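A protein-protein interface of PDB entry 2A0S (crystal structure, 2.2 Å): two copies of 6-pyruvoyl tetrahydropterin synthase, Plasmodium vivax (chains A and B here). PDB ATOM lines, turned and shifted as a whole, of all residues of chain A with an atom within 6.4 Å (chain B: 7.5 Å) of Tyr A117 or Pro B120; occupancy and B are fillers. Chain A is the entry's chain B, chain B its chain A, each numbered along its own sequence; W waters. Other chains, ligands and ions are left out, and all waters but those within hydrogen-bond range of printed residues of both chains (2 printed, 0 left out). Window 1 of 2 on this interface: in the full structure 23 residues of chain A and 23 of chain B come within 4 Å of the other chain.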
ATOM      1  N   PHE A  37     -28.042 -30.391  28.202  1.00  0.00           N
ATOM      2  CA  PHE A  37     -28.337 -30.262  29.628  1.00  0.00           C
ATOM      3  C   PHE A  37     -29.845 -30.252  29.865  1.00  0.00           C
ATOM      4  O   PHE A  37     -30.607 -29.693  29.072  1.00  0.00           O
ATOM      5  CB  PHE A  37     -27.645 -29.042  30.268  1.00  0.00           C
ATOM      6  CG  PHE A  37     -28.115 -27.710  29.746  1.00  0.00           C
ATOM      7  CD1 PHE A  37     -29.166 -27.034  30.366  1.00  0.00           C
ATOM      8  CD2 PHE A  37     -27.487 -27.113  28.657  1.00  0.00           C
ATOM      9  CE1 PHE A  37     -29.598 -25.795  29.895  1.00  0.00           C
ATOM     10  CE2 PHE A  37     -27.909 -25.875  28.179  1.00  0.00           C
ATOM     11  CZ  PHE A  37     -28.968 -25.214  28.799  1.00  0.00           C
ATOM     12  N   ARG A  44     -31.934 -26.818  36.849  1.00  0.00           N
ATOM     13  CA  ARG A  44     -31.041 -26.710  35.703  1.00  0.00           C
ATOM     14  C   ARG A  44     -29.706 -27.365  36.039  1.00  0.00           C
ATOM     15  O   ARG A  44     -29.144 -27.129  37.110  1.00  0.00           O
ATOM     16  CB  ARG A  44     -30.828 -25.241  35.325  1.00  0.00           C
ATOM     17  CG  ARG A  44     -29.947 -25.029  34.099  1.00  0.00           C
ATOM     18  CD  ARG A  44     -29.347 -23.632  34.070  1.00  0.00           C
ATOM     19  NE  ARG A  44     -28.356 -23.415  35.125  1.00  0.00           N
ATOM     20  CZ  ARG A  44     -27.052 -23.644  34.999  1.00  0.00           C
ATOM     21  NH1 ARG A  44     -26.558 -24.111  33.861  1.00  0.00           N
ATOM     22  NH2 ARG A  44     -26.236 -23.412  36.016  1.00  0.00           N
ATOM     23  N   GLU A  45     -29.209 -28.190  35.123  1.00  0.00           N
ATOM     24  CA  GLU A  45     -27.895 -28.808  35.286  1.00  0.00           C
ATOM     25  C   GLU A  45     -26.862 -28.193  34.344  1.00  0.00           C
ATOM     26  O   GLU A  45     -27.214 -27.505  33.381  1.00  0.00           O
ATOM     27  CB  GLU A  45     -27.975 -30.322  35.089  1.00  0.00           C
ATOM     28  CG  GLU A  45     -28.340 -30.762  33.683  1.00  0.00           C
ATOM     29  CD  GLU A  45     -28.664 -32.239  33.599  1.00  0.00           C
ATOM     30  OE1 GLU A  45     -28.888 -32.865  34.655  1.00  0.00           O
ATOM     31  OE2 GLU A  45     -28.705 -32.773  32.472  1.00  0.00           O
ATOM     32  N   THR A  46     -25.589 -28.447  34.632  1.00  0.00           N
ATOM     33  CA  THR A  46     -24.494 -27.915  33.828  1.00  0.00           C
ATOM     34  C   THR A  46     -24.366 -28.648  32.494  1.00  0.00           C
ATOM     35  O   THR A  46     -24.793 -29.800  32.360  1.00  0.00           O
ATOM     36  CB  THR A  46     -23.149 -27.970  34.584  1.00  0.00           C
ATOM     37  OG1 THR A  46     -22.922 -29.300  35.061  1.00  0.00           O
ATOM     38  CG2 THR A  46     -23.151 -27.006  35.767  1.00  0.00           C
ATOM     39  N   LEU A  47     -23.783 -27.966  31.512  1.00  0.00           N
ATOM     40  CA  LEU A  47     -23.526 -28.543  30.198  1.00  0.00           C
ATOM     41  C   LEU A  47     -22.597 -29.751  30.294  1.00  0.00           C
ATOM     42  O   LEU A  47     -21.540 -29.692  30.925  1.00  0.00           O
ATOM     43  CB  LEU A  47     -22.932 -27.492  29.252  1.00  0.00           C
ATOM     44  CG  LEU A  47     -22.515 -27.936  27.843  1.00  0.00           C
ATOM     45  CD1 LEU A  47     -23.726 -28.239  26.969  1.00  0.00           C
ATOM     46  CD2 LEU A  47     -21.634 -26.886  27.186  1.00  0.00           C
ATOM     47  N   PHE A  89     -24.878 -30.250  19.812  1.00  0.00           N
ATOM     48  CA  PHE A  89     -25.597 -29.942  21.043  1.00  0.00           C
ATOM     49  C   PHE A  89     -27.085 -30.144  20.773  1.00  0.00           C
ATOM     50  O   PHE A  89     -27.627 -29.599  19.809  1.00  0.00           O
ATOM     51  CB  PHE A  89     -25.318 -28.506  21.510  1.00  0.00           C
ATOM     52  CG  PHE A  89     -26.216 -28.038  22.630  1.00  0.00           C
ATOM     53  CD1 PHE A  89     -25.940 -28.377  23.954  1.00  0.00           C
ATOM     54  CD2 PHE A  89     -27.337 -27.256  22.361  1.00  0.00           C
ATOM     55  CE1 PHE A  89     -26.768 -27.947  24.989  1.00  0.00           C
ATOM     56  CE2 PHE A  89     -28.173 -26.823  23.389  1.00  0.00           C
ATOM     57  CZ  PHE A  89     -27.888 -27.169  24.706  1.00  0.00           C
ATOM     58  N   PHE A 107     -26.992 -19.571  18.325  1.00  0.00           N
ATOM     59  CA  PHE A 107     -28.125 -19.663  19.235  1.00  0.00           C
ATOM     60  C   PHE A 107     -27.663 -19.222  20.618  1.00  0.00           C
ATOM     61  O   PHE A 107     -26.685 -19.748  21.152  1.00  0.00           O
ATOM     62  CB  PHE A 107     -28.682 -21.087  19.301  1.00  0.00           C
ATOM     63  CG  PHE A 107     -29.502 -21.486  18.103  1.00  0.00           C
ATOM     64  CD1 PHE A 107     -29.163 -22.611  17.359  1.00  0.00           C
ATOM     65  CD2 PHE A 107     -30.621 -20.746  17.725  1.00  0.00           C
ATOM     66  CE1 PHE A 107     -29.919 -22.995  16.256  1.00  0.00           C
ATOM     67  CE2 PHE A 107     -31.383 -21.120  16.619  1.00  0.00           C
ATOM     68  CZ  PHE A 107     -31.031 -22.246  15.883  1.00  0.00           C
ATOM     69  N   LYS A 108     -28.359 -18.240  21.177  1.00  0.00           N
ATOM     70  CA  LYS A 108     -28.109 -17.779  22.534  1.00  0.00           C
ATOM     71  C   LYS A 108     -29.206 -18.315  23.448  1.00  0.00           C
ATOM     72  O   LYS A 108     -30.393 -18.072  23.220  1.00  0.00           O
ATOM     73  CB  LYS A 108     -28.058 -16.249  22.577  1.00  0.00           C
ATOM     74  CG  LYS A 108     -27.755 -15.659  23.945  1.00  0.00           C
ATOM     75  CD  LYS A 108     -27.658 -14.145  23.868  1.00  0.00           C
ATOM     76  CE  LYS A 108     -27.567 -13.529  25.251  1.00  0.00           C
ATOM     77  NZ  LYS A 108     -27.420 -12.047  25.186  1.00  0.00           N
ATOM     78  N   ILE A 109     -28.798 -19.050  24.478  1.00  0.00           N
ATOM     79  CA  ILE A 109     -29.735 -19.680  25.401  1.00  0.00           C
ATOM     80  C   ILE A 109     -29.632 -19.061  26.792  1.00  0.00           C
ATOM     81  O   ILE A 109     -28.575 -19.107  27.426  1.00  0.00           O
ATOM     82  CB  ILE A 109     -29.522 -21.212  25.473  1.00  0.00           C
ATOM     83  CG1 ILE A 109     -29.612 -21.826  24.072  1.00  0.00           C
ATOM     84  CG2 ILE A 109     -30.535 -21.856  26.423  1.00  0.00           C
ATOM     85  CD1 ILE A 109     -28.956 -23.180  23.947  1.00  0.00           C
ATOM     86  N   THR A 110     -30.737 -18.474  27.248  1.00  0.00           N
ATOM     87  CA  THR A 110     -30.822 -17.896  28.586  1.00  0.00           C
ATOM     88  C   THR A 110     -31.746 -18.741  29.457  1.00  0.00           C
ATOM     89  O   THR A 110     -32.889 -19.022  29.082  1.00  0.00           O
ATOM     90  CB  THR A 110     -31.320 -16.432  28.549  1.00  0.00           C
ATOM     91  OG1 THR A 110     -30.574 -15.694  27.574  1.00  0.00           O
ATOM     92  CG2 THR A 110     -31.154 -15.765  29.916  1.00  0.00           C
ATOM     93  N   CYS A 111     -31.236 -19.143  30.619  1.00  0.00           N
ATOM     94  CA  CYS A 111     -31.966 -20.000  31.548  1.00  0.00           C
ATOM     95  C   CYS A 111     -32.726 -19.178  32.597  1.00  0.00           C
ATOM     96  O   CYS A 111     -32.599 -17.949  32.639  1.00  0.00           O
ATOM     97  CB  CYS A 111     -30.998 -20.980  32.220  1.00  0.00           C
ATOM     98  SG  CYS A 111     -29.978 -21.938  31.067  1.00  0.00           S
ATOM     99  N   SER A 115     -28.326 -17.764  33.713  1.00  0.00           N
ATOM    100  CA  SER A 115     -27.110 -18.281  33.084  1.00  0.00           C
ATOM    101  C   SER A 115     -27.255 -18.249  31.560  1.00  0.00           C
ATOM    102  O   SER A 115     -28.336 -18.518  31.025  1.00  0.00           O
ATOM    103  CB  SER A 115     -26.774 -19.686  33.588  1.00  0.00           C
ATOM    104  OG  SER A 115     -27.798 -20.609  33.269  1.00  0.00           O
ATOM    105  N   GLU A 116     -26.163 -17.913  30.877  1.00  0.00           N
ATOM    106  CA  GLU A 116     -26.174 -17.706  29.428  1.00  0.00           C
ATOM    107  C   GLU A 116     -25.259 -18.673  28.684  1.00  0.00           C
ATOM    108  O   GLU A 116     -24.113 -18.894  29.082  1.00  0.00           O
ATOM    109  CB  GLU A 116     -25.762 -16.269  29.092  1.00  0.00           C
ATOM    110  CG  GLU A 116     -26.802 -15.210  29.420  1.00  0.00           C
ATOM    111  CD  GLU A 116     -26.252 -13.799  29.306  1.00  0.00           C
ATOM    112  OE1 GLU A 116     -25.301 -13.461  30.044  1.00  0.00           O
ATOM    113  OE2 GLU A 116     -26.777 -13.022  28.483  1.00  0.00           O
ATOM    114  N   TYR A 117     -25.780 -19.235  27.596  1.00  0.00           N
ATOM    115  CA  TYR A 117     -25.003 -20.085  26.695  1.00  0.00           C
ATOM    116  C   TYR A 117     -25.055 -19.487  25.295  1.00  0.00           C
ATOM    117  O   TYR A 117     -26.037 -18.837  24.929  1.00  0.00           O
ATOM    118  CB  TYR A 117     -25.569 -21.507  26.649  1.00  0.00           C
ATOM    119  CG  TYR A 117     -25.527 -22.251  27.962  1.00  0.00           C
ATOM    120  CD1 TYR A 117     -26.541 -22.092  28.906  1.00  0.00           C
ATOM    121  CD2 TYR A 117     -24.484 -23.128  28.254  1.00  0.00           C
ATOM    122  CE1 TYR A 117     -26.512 -22.776  30.112  1.00  0.00           C
ATOM    123  CE2 TYR A 117     -24.447 -23.821  29.457  1.00  0.00           C
ATOM    124  CZ  TYR A 117     -25.463 -23.635  30.381  1.00  0.00           C
ATOM    125  OH  TYR A 117     -25.441 -24.312  31.575  1.00  0.00           O
ATOM    126  N   SER A 118     -24.000 -19.707  24.516  1.00  0.00           N
ATOM    127  CA  SER A 118     -23.990 -19.310  23.112  1.00  0.00           C
ATOM    128  C   SER A 118     -23.221 -20.325  22.277  1.00  0.00           C
ATOM    129  O   SER A 118     -22.034 -20.557  22.508  1.00  0.00           O
ATOM    130  CB  SER A 118     -23.400 -17.906  22.940  1.00  0.00           C
ATOM    131  OG  SER A 118     -23.553 -17.452  21.606  1.00  0.00           O
ATOM    132  N   PHE A 119     -23.916 -20.941  21.324  1.00  0.00           N
ATOM    133  CA  PHE A 119     -23.304 -21.897  20.404  1.00  0.00           C
ATOM    134  C   PHE A 119     -23.570 -21.468  18.968  1.00  0.00           C
ATOM    135  O   PHE A 119     -24.619 -20.887  18.693  1.00  0.00           O
ATOM    136  CB  PHE A 119     -23.884 -23.307  20.585  1.00  0.00           C
ATOM    137  CG  PHE A 119     -24.116 -23.717  22.014  1.00  0.00           C
ATOM    138  CD1 PHE A 119     -25.405 -23.978  22.467  1.00  0.00           C
ATOM    139  CD2 PHE A 119     -23.055 -23.876  22.897  1.00  0.00           C
ATOM    140  CE1 PHE A 119     -25.635 -24.375  23.780  1.00  0.00           C
ATOM    141  CE2 PHE A 119     -23.281 -24.273  24.215  1.00  0.00           C
ATOM    142  CZ  PHE A 119     -24.571 -24.523  24.656  1.00  0.00           C
ATOM    143  N   LEU B  47     -19.341 -28.877  18.637  1.00  0.00           N
ATOM    144  CA  LEU B  47     -19.553 -29.246  20.032  1.00  0.00           C
ATOM    145  C   LEU B  47     -20.372 -30.530  20.148  1.00  0.00           C
ATOM    146  O   LEU B  47     -21.423 -30.673  19.521  1.00  0.00           O
ATOM    147  CB  LEU B  47     -20.241 -28.106  20.792  1.00  0.00           C
ATOM    148  CG  LEU B  47     -20.600 -28.324  22.268  1.00  0.00           C
ATOM    149  CD1 LEU B  47     -19.355 -28.397  23.143  1.00  0.00           C
ATOM    150  CD2 LEU B  47     -21.527 -27.225  22.752  1.00  0.00           C
ATOM    151  N   HIS B  88     -19.307 -31.536  32.965  1.00  0.00           N
ATOM    152  CA  HIS B  88     -18.721 -30.255  32.570  1.00  0.00           C
ATOM    153  C   HIS B  88     -18.318 -30.242  31.099  1.00  0.00           C
ATOM    154  O   HIS B  88     -18.199 -31.293  30.471  1.00  0.00           O
ATOM    155  CB  HIS B  88     -17.497 -29.929  33.434  1.00  0.00           C
ATOM    156  CG  HIS B  88     -17.827 -29.601  34.857  1.00  0.00           C
ATOM    157  ND1 HIS B  88     -17.640 -30.496  35.888  1.00  0.00           N
ATOM    158  CD2 HIS B  88     -18.331 -28.478  35.419  1.00  0.00           C
ATOM    159  CE1 HIS B  88     -18.016 -29.938  37.025  1.00  0.00           C
ATOM    160  NE2 HIS B  88     -18.439 -28.713  36.768  1.00  0.00           N
ATOM    161  N   PHE B  89     -18.124 -29.044  30.554  1.00  0.00           N
ATOM    162  CA  PHE B  89     -17.425 -28.886  29.284  1.00  0.00           C
ATOM    163  C   PHE B  89     -15.927 -28.911  29.573  1.00  0.00           C
ATOM    164  O   PHE B  89     -15.441 -28.160  30.421  1.00  0.00           O
ATOM    165  CB  PHE B  89     -17.828 -27.578  28.589  1.00  0.00           C
ATOM    166  CG  PHE B  89     -16.960 -27.220  27.408  1.00  0.00           C
ATOM    167  CD1 PHE B  89     -17.180 -27.799  26.159  1.00  0.00           C
ATOM    168  CD2 PHE B  89     -15.924 -26.297  27.544  1.00  0.00           C
ATOM    169  CE1 PHE B  89     -16.376 -27.469  25.067  1.00  0.00           C
ATOM    170  CE2 PHE B  89     -15.117 -25.961  26.458  1.00  0.00           C
ATOM    171  CZ  PHE B  89     -15.345 -26.548  25.218  1.00  0.00           C
ATOM    172  N   VAL B 103     -15.566 -13.327  30.190  1.00  0.00           N
ATOM    173  CA  VAL B 103     -16.604 -12.310  30.054  1.00  0.00           C
ATOM    174  C   VAL B 103     -17.619 -12.512  31.172  1.00  0.00           C
ATOM    175  O   VAL B 103     -18.361 -13.497  31.174  1.00  0.00           O
ATOM    176  CB  VAL B 103     -17.306 -12.370  28.671  1.00  0.00           C
ATOM    177  CG1 VAL B 103     -18.386 -11.298  28.561  1.00  0.00           C
ATOM    178  CG2 VAL B 103     -16.294 -12.215  27.545  1.00  0.00           C
ATOM    179  N   ASP B 105     -19.283 -13.831  34.123  1.00  0.00           N
ATOM    180  CA  ASP B 105     -19.192 -15.147  34.760  1.00  0.00           C
ATOM    181  C   ASP B 105     -19.142 -16.272  33.724  1.00  0.00           C
ATOM    182  O   ASP B 105     -19.462 -17.428  34.020  1.00  0.00           O
ATOM    183  CB  ASP B 105     -20.355 -15.350  35.738  1.00  0.00           C
ATOM    184  CG  ASP B 105     -20.381 -14.304  36.843  1.00  0.00           C
ATOM    185  OD1 ASP B 105     -19.308 -13.987  37.403  1.00  0.00           O
ATOM    186  OD2 ASP B 105     -21.481 -13.803  37.157  1.00  0.00           O
ATOM    187  N   ASN B 106     -18.726 -15.919  32.510  1.00  0.00           N
ATOM    188  CA  ASN B 106     -18.639 -16.864  31.402  1.00  0.00           C
ATOM    189  C   ASN B 106     -17.234 -16.984  30.820  1.00  0.00           C
ATOM    190  O   ASN B 106     -16.413 -16.072  30.950  1.00  0.00           O
ATOM    191  CB  ASN B 106     -19.609 -16.464  30.282  1.00  0.00           C
ATOM    192  CG  ASN B 106     -21.038 -16.906  30.550  1.00  0.00           C
ATOM    193  OD1 ASN B 106     -21.553 -16.765  31.660  1.00  0.00           O
ATOM    194  ND2 ASN B 106     -21.692 -17.434  29.522  1.00  0.00           N
ATOM    195  N   PHE B 107     -16.968 -18.126  30.190  1.00  0.00           N
ATOM    196  CA  PHE B 107     -15.825 -18.270  29.301  1.00  0.00           C
ATOM    197  C   PHE B 107     -16.311 -18.110  27.866  1.00  0.00           C
ATOM    198  O   PHE B 107     -17.227 -18.811  27.430  1.00  0.00           O
ATOM    199  CB  PHE B 107     -15.148 -19.636  29.468  1.00  0.00           C
ATOM    200  CG  PHE B 107     -14.316 -19.764  30.717  1.00  0.00           C
ATOM    201  CD1 PHE B 107     -14.530 -20.817  31.600  1.00  0.00           C
ATOM    202  CD2 PHE B 107     -13.312 -18.841  31.007  1.00  0.00           C
ATOM    203  CE1 PHE B 107     -13.763 -20.951  32.753  1.00  0.00           C
ATOM    204  CE2 PHE B 107     -12.540 -18.964  32.161  1.00  0.00           C
ATOM    205  CZ  PHE B 107     -12.765 -20.021  33.035  1.00  0.00           C
ATOM    206  N   LYS B 108     -15.707 -17.170  27.147  1.00  0.00           N
ATOM    207  CA  LYS B 108     -15.984 -16.977  25.730  1.00  0.00           C
ATOM    208  C   LYS B 108     -14.838 -17.572  24.916  1.00  0.00           C
ATOM    209  O   LYS B 108     -13.677 -17.190  25.090  1.00  0.00           O
ATOM    210  CB  LYS B 108     -16.161 -15.489  25.417  1.00  0.00           C
ATOM    211  CG  LYS B 108     -16.542 -15.180  23.974  1.00  0.00           C
ATOM    212  CD  LYS B 108     -16.769 -13.689  23.787  1.00  0.00           C
ATOM    213  CE  LYS B 108     -16.902 -13.327  22.321  1.00  0.00           C
ATOM    214  NZ  LYS B 108     -17.204 -11.878  22.134  1.00  0.00           N
ATOM    215  N   TYR B 117     -18.140 -19.478  21.012  1.00  0.00           N
ATOM    216  CA  TYR B 117     -18.850 -20.220  22.051  1.00  0.00           C
ATOM    217  C   TYR B 117     -18.859 -19.389  23.326  1.00  0.00           C
ATOM    218  O   TYR B 117     -17.940 -18.604  23.568  1.00  0.00           O
ATOM    219  CB  TYR B 117     -18.166 -21.559  22.340  1.00  0.00           C
ATOM    220  CG  TYR B 117     -18.133 -22.522  21.178  1.00  0.00           C
ATOM    221  CD1 TYR B 117     -17.134 -22.439  20.207  1.00  0.00           C
ATOM    222  CD2 TYR B 117     -19.086 -23.532  21.060  1.00  0.00           C
ATOM    223  CE1 TYR B 117     -17.093 -23.325  19.141  1.00  0.00           C
ATOM    224  CE2 TYR B 117     -19.051 -24.428  20.000  1.00  0.00           C
ATOM    225  CZ  TYR B 117     -18.053 -24.316  19.044  1.00  0.00           C
ATOM    226  OH  TYR B 117     -18.010 -25.193  17.990  1.00  0.00           O
ATOM    227  N   SER B 118     -19.897 -19.561  24.140  1.00  0.00           N
ATOM    228  CA  SER B 118     -19.945 -18.939  25.458  1.00  0.00           C
ATOM    229  C   SER B 118     -20.633 -19.856  26.460  1.00  0.00           C
ATOM    230  O   SER B 118     -21.799 -20.214  26.285  1.00  0.00           O
ATOM    231  CB  SER B 118     -20.637 -17.573  25.400  1.00  0.00           C
ATOM    232  OG  SER B 118     -20.507 -16.881  26.633  1.00  0.00           O
ATOM    233  N   PHE B 119     -19.891 -20.251  27.494  1.00  0.00           N
ATOM    234  CA  PHE B 119     -20.425 -21.084  28.569  1.00  0.00           C
ATOM    235  C   PHE B 119     -20.205 -20.397  29.911  1.00  0.00           C
ATOM    236  O   PHE B 119     -19.207 -19.692  30.079  1.00  0.00           O
ATOM    237  CB  PHE B 119     -19.729 -22.455  28.627  1.00  0.00           C
ATOM    238  CG  PHE B 119     -19.500 -23.105  27.288  1.00  0.00           C
ATOM    239  CD1 PHE B 119     -18.209 -23.413  26.873  1.00  0.00           C
ATOM    240  CD2 PHE B 119     -20.563 -23.437  26.457  1.00  0.00           C
ATOM    241  CE1 PHE B 119     -17.979 -24.030  25.643  1.00  0.00           C
ATOM    242  CE2 PHE B 119     -20.337 -24.052  25.224  1.00  0.00           C
ATOM    243  CZ  PHE B 119     -19.044 -24.349  24.819  1.00  0.00           C
ATOM    244  N   PRO B 120     -21.117 -20.614  30.881  1.00  0.00           N
ATOM    245  CA  PRO B 120     -20.829 -20.194  32.252  1.00  0.00           C
ATOM    246  C   PRO B 120     -19.557 -20.877  32.751  1.00  0.00           C
ATOM    247  O   PRO B 120     -19.310 -22.037  32.412  1.00  0.00           O
ATOM    248  CB  PRO B 120     -22.041 -20.703  33.038  1.00  0.00           C
ATOM    249  CG  PRO B 120     -23.129 -20.819  32.028  1.00  0.00           C
ATOM    250  CD  PRO B 120     -22.446 -21.241  30.766  1.00  0.00           C
ATOM    251  N   LYS B 121     -18.757 -20.159  33.535  1.00  0.00           N
ATOM    252  CA  LYS B 121     -17.497 -20.690  34.063  1.00  0.00           C
ATOM    253  C   LYS B 121     -17.685 -21.973  34.880  1.00  0.00           C
ATOM    254  O   LYS B 121     -16.856 -22.886  34.799  1.00  0.00           O
ATOM    255  CB  LYS B 121     -16.774 -19.638  34.909  1.00  0.00           C
ATOM    256  CG  LYS B 121     -16.189 -18.474  34.123  1.00  0.00           C
ATOM    257  CD  LYS B 121     -15.634 -17.420  35.068  1.00  0.00           C
ATOM    258  CE  LYS B 121     -15.080 -16.222  34.317  1.00  0.00           C
ATOM    259  NZ  LYS B 121     -14.557 -15.191  35.260  1.00  0.00           N
ATOM    260  N   ARG B 122     -18.777 -22.032  35.646  1.00  0.00           N
ATOM    261  CA  ARG B 122     -19.075 -23.179  36.506  1.00  0.00           C
ATOM    262  C   ARG B 122     -19.422 -24.441  35.705  1.00  0.00           C
ATOM    263  O   ARG B 122     -19.339 -25.555  36.225  1.00  0.00           O
ATOM    264  CB  ARG B 122     -20.203 -22.828  37.482  1.00  0.00           C
ATOM    265  CG  ARG B 122     -20.231 -23.671  38.752  1.00  0.00           C
ATOM    266  CD  ARG B 122     -21.127 -23.049  39.815  1.00  0.00           C
ATOM    267  NE  ARG B 122     -20.540 -21.839  40.391  1.00  0.00           N
ATOM    268  CZ  ARG B 122     -21.165 -21.023  41.236  1.00  0.00           C
ATOM    269  NH1 ARG B 122     -20.538 -19.949  41.702  1.00  0.00           N
ATOM    270  NH2 ARG B 122     -22.411 -21.271  41.618  1.00  0.00           N
ATOM    271  N   ASP B 123     -19.803 -24.254  34.442  1.00  0.00           N
ATOM    272  CA  ASP B 123     -20.099 -25.363  33.534  1.00  0.00           C
ATOM    273  C   ASP B 123     -18.831 -25.952  32.926  1.00  0.00           C
ATOM    274  O   ASP B 123     -18.863 -27.041  32.352  1.00  0.00           O
ATOM    275  CB  ASP B 123     -21.032 -24.905  32.411  1.00  0.00           C
ATOM    276  CG  ASP B 123     -22.472 -24.788  32.859  1.00  0.00           C
ATOM    277  OD1 ASP B 123     -22.736 -24.146  33.898  1.00  0.00           O
ATOM    278  OD2 ASP B 123     -23.346 -25.335  32.161  1.00  0.00           O
ATOM    279  N   CYS B 124     -17.726 -25.221  33.044  1.00  0.00           N
ATOM    280  CA  CYS B 124     -16.457 -25.627  32.453  1.00  0.00           C
ATOM    281  C   CYS B 124     -15.491 -26.150  33.505  1.00  0.00           C
ATOM    282  O   CYS B 124     -15.491 -25.692  34.651  1.00  0.00           O
ATOM    283  CB  CYS B 124     -15.807 -24.456  31.710  1.00  0.00           C
ATOM    284  SG  CYS B 124     -16.793 -23.766  30.365  1.00  0.00           S
ATOM    285  N   VAL B 125     -14.674 -27.116  33.103  1.00  0.00           N
ATOM    286  CA  VAL B 125     -13.542 -27.544  33.909  1.00  0.00           C
ATOM    287  C   VAL B 125     -12.252 -27.219  33.149  1.00  0.00           C
ATOM    288  O   VAL B 125     -12.011 -27.732  32.052  1.00  0.00           O
ATOM    289  CB  VAL B 125     -13.650 -29.041  34.350  1.00  0.00           C
ATOM    290  CG1 VAL B 125     -13.728 -29.991  33.148  1.00  0.00           C
ATOM    291  CG2 VAL B 125     -12.505 -29.419  35.284  1.00  0.00           C
HETATM  292  O   HOH W   1     -21.395 -29.743  37.861  1.00  0.00           O
HETATM  293  O   HOH W   2     -24.001 -17.231  32.459  1.00  0.00           O
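The backbone NH (N) of Phe A89 sits at hydrogen-bond distance from the backbone carbonyl oxygen (O) of Leu B47, 3.5 Å away.
The backbone NH (N) of Phe B89 is in hydrogen-bond range of the backbone carbonyl oxygen (O) of Leu A47 (3.5 Å).
The backbone carbonyl oxygen of Glu A116 lies within hydrogen-bond range of the side-chain amide nitrogen of Asn B106 (2.9 Å).
The backbone NH (N) of Ser B118 lies within hydrogen-bond range of the backbone carbonyl oxygen (O) of Ser A118 (2.9 Å).
OD1 of Asp B123 lies within salt-bridge range of NH1 of Arg A44, at 3.8 Å.
N of Leu A47 is in hydrogen-bond range of OD2 of Asp B123 (2.7 Å).
OD2 of Asp B123 is in hydrogen-bond range of OH of Tyr A117, 2.4 Å away.
A ring nitrogen (NE2) of His B88 lies close to the backbone carbonyl oxygen of Arg B122.
N of Phe B89 lies within hydrogen-bond range of O of Asp B123 (2.8 Å).
The backbone NH of Val B125 is in hydrogen-bond range of the backbone carbonyl oxygen of Phe B89 (3.0 Å).
O of Pro B120 is in hydrogen-bond range of SG of Cys B124 (3.7 Å).
The guanidinium group of Arg A44 is in hydrogen-bond range of the side-chain hydroxyl of Ser A115.
NZ of Lys A108 is in salt-bridge range of OE2 of Glu A116 (3.5 Å).
Among the printed residues, merely in contact across the chains: Thr A46 with Asp B123 (3.3 Å), Leu A47 with His B88 (3.3 Å), Leu A47 with Phe B119 (3.7 Å), Glu A116 with Ser B118 (3.9 Å), Glu A116 with Pro B120 (3.3 Å), Tyr A117 with Ser B118 (3.2 Å), Tyr A117 with Pro B120 (3.5 Å), Ser A118 with Tyr B117 (3.2 Å), Phe A119 with Leu B47 (3.7 Å) and Phe A119 with Phe B119 (3.1 Å).
Of the printed residues of chain B, Glu A116 touches Asn B106 (2.9 Å), Ser B118 (3.9 Å) and Pro B120 (3.3 Å).
Tyr A117 touches just these residues of chain B: Ser B118 (3.2 Å), Pro B120 (3.5 Å) and Asp B123 (2.4 Å).
Printed residues of chain A within 4 Å of Leu B47: Phe A89 and Phe A119.
Of the printed residues of chain A, His B88 touches Leu A47 (3.3 Å).
Printed residues of chain A within 4 Å of Phe B89: Leu A47 (3.5 Å).
Of the printed residues of chain A, Asn B106 touches Glu A116 (2.9 Å).
Phe B107 touches none of the printed residues of chain A.
The nearest residue of chain B that does not touch Tyr A117 is Phe B119 (4.3 Å).
The nearest printed residue of chain A that does not touch Asn B106 is Tyr A117 (4.9 Å).
Hydrophobic or aromatic side chains of chain A that line the printed part of chain B: Leu A47, Tyr A117 and Phe A119.
Hydrophobic or aromatic side chains of chain B within 4 Å of the printed part of chain A: Leu B47, Tyr B117, Phe B119 and Pro B120.
Among the printed residues, Asp or Glu carboxylates within 4 Å of a Lys or Arg side-chain nitrogen of the other chain: Arg A44 with Asp B123 (3.8 Å).
Leu A47 touches Phe B119, and with the chains exchanged Phe A119 touches Leu B47.
Tyr A117 touches Ser B118, and with the chains exchanged Ser A118 touches Tyr B117.
Ser B118 touches its own counterpart, Ser A118.
Phe A119 touches its own counterpart, Phe B119.
Positions printed for both chains: 47, 89, 107, 108, 117, 118 and 119.
Of the 17 pairs that touch across the chains among the printed residues, 8 have their exchanged pair printed and touching as well.
Water W2 bridges OD1 of Asn B106 (2.6 Å) and N of Glu A116 (2.8 Å).
Water W1 lies within hydrogen-bond range of the side-chain hydroxyl (OG1) of Thr A46 and a ring nitrogen (NE2) of His B88.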
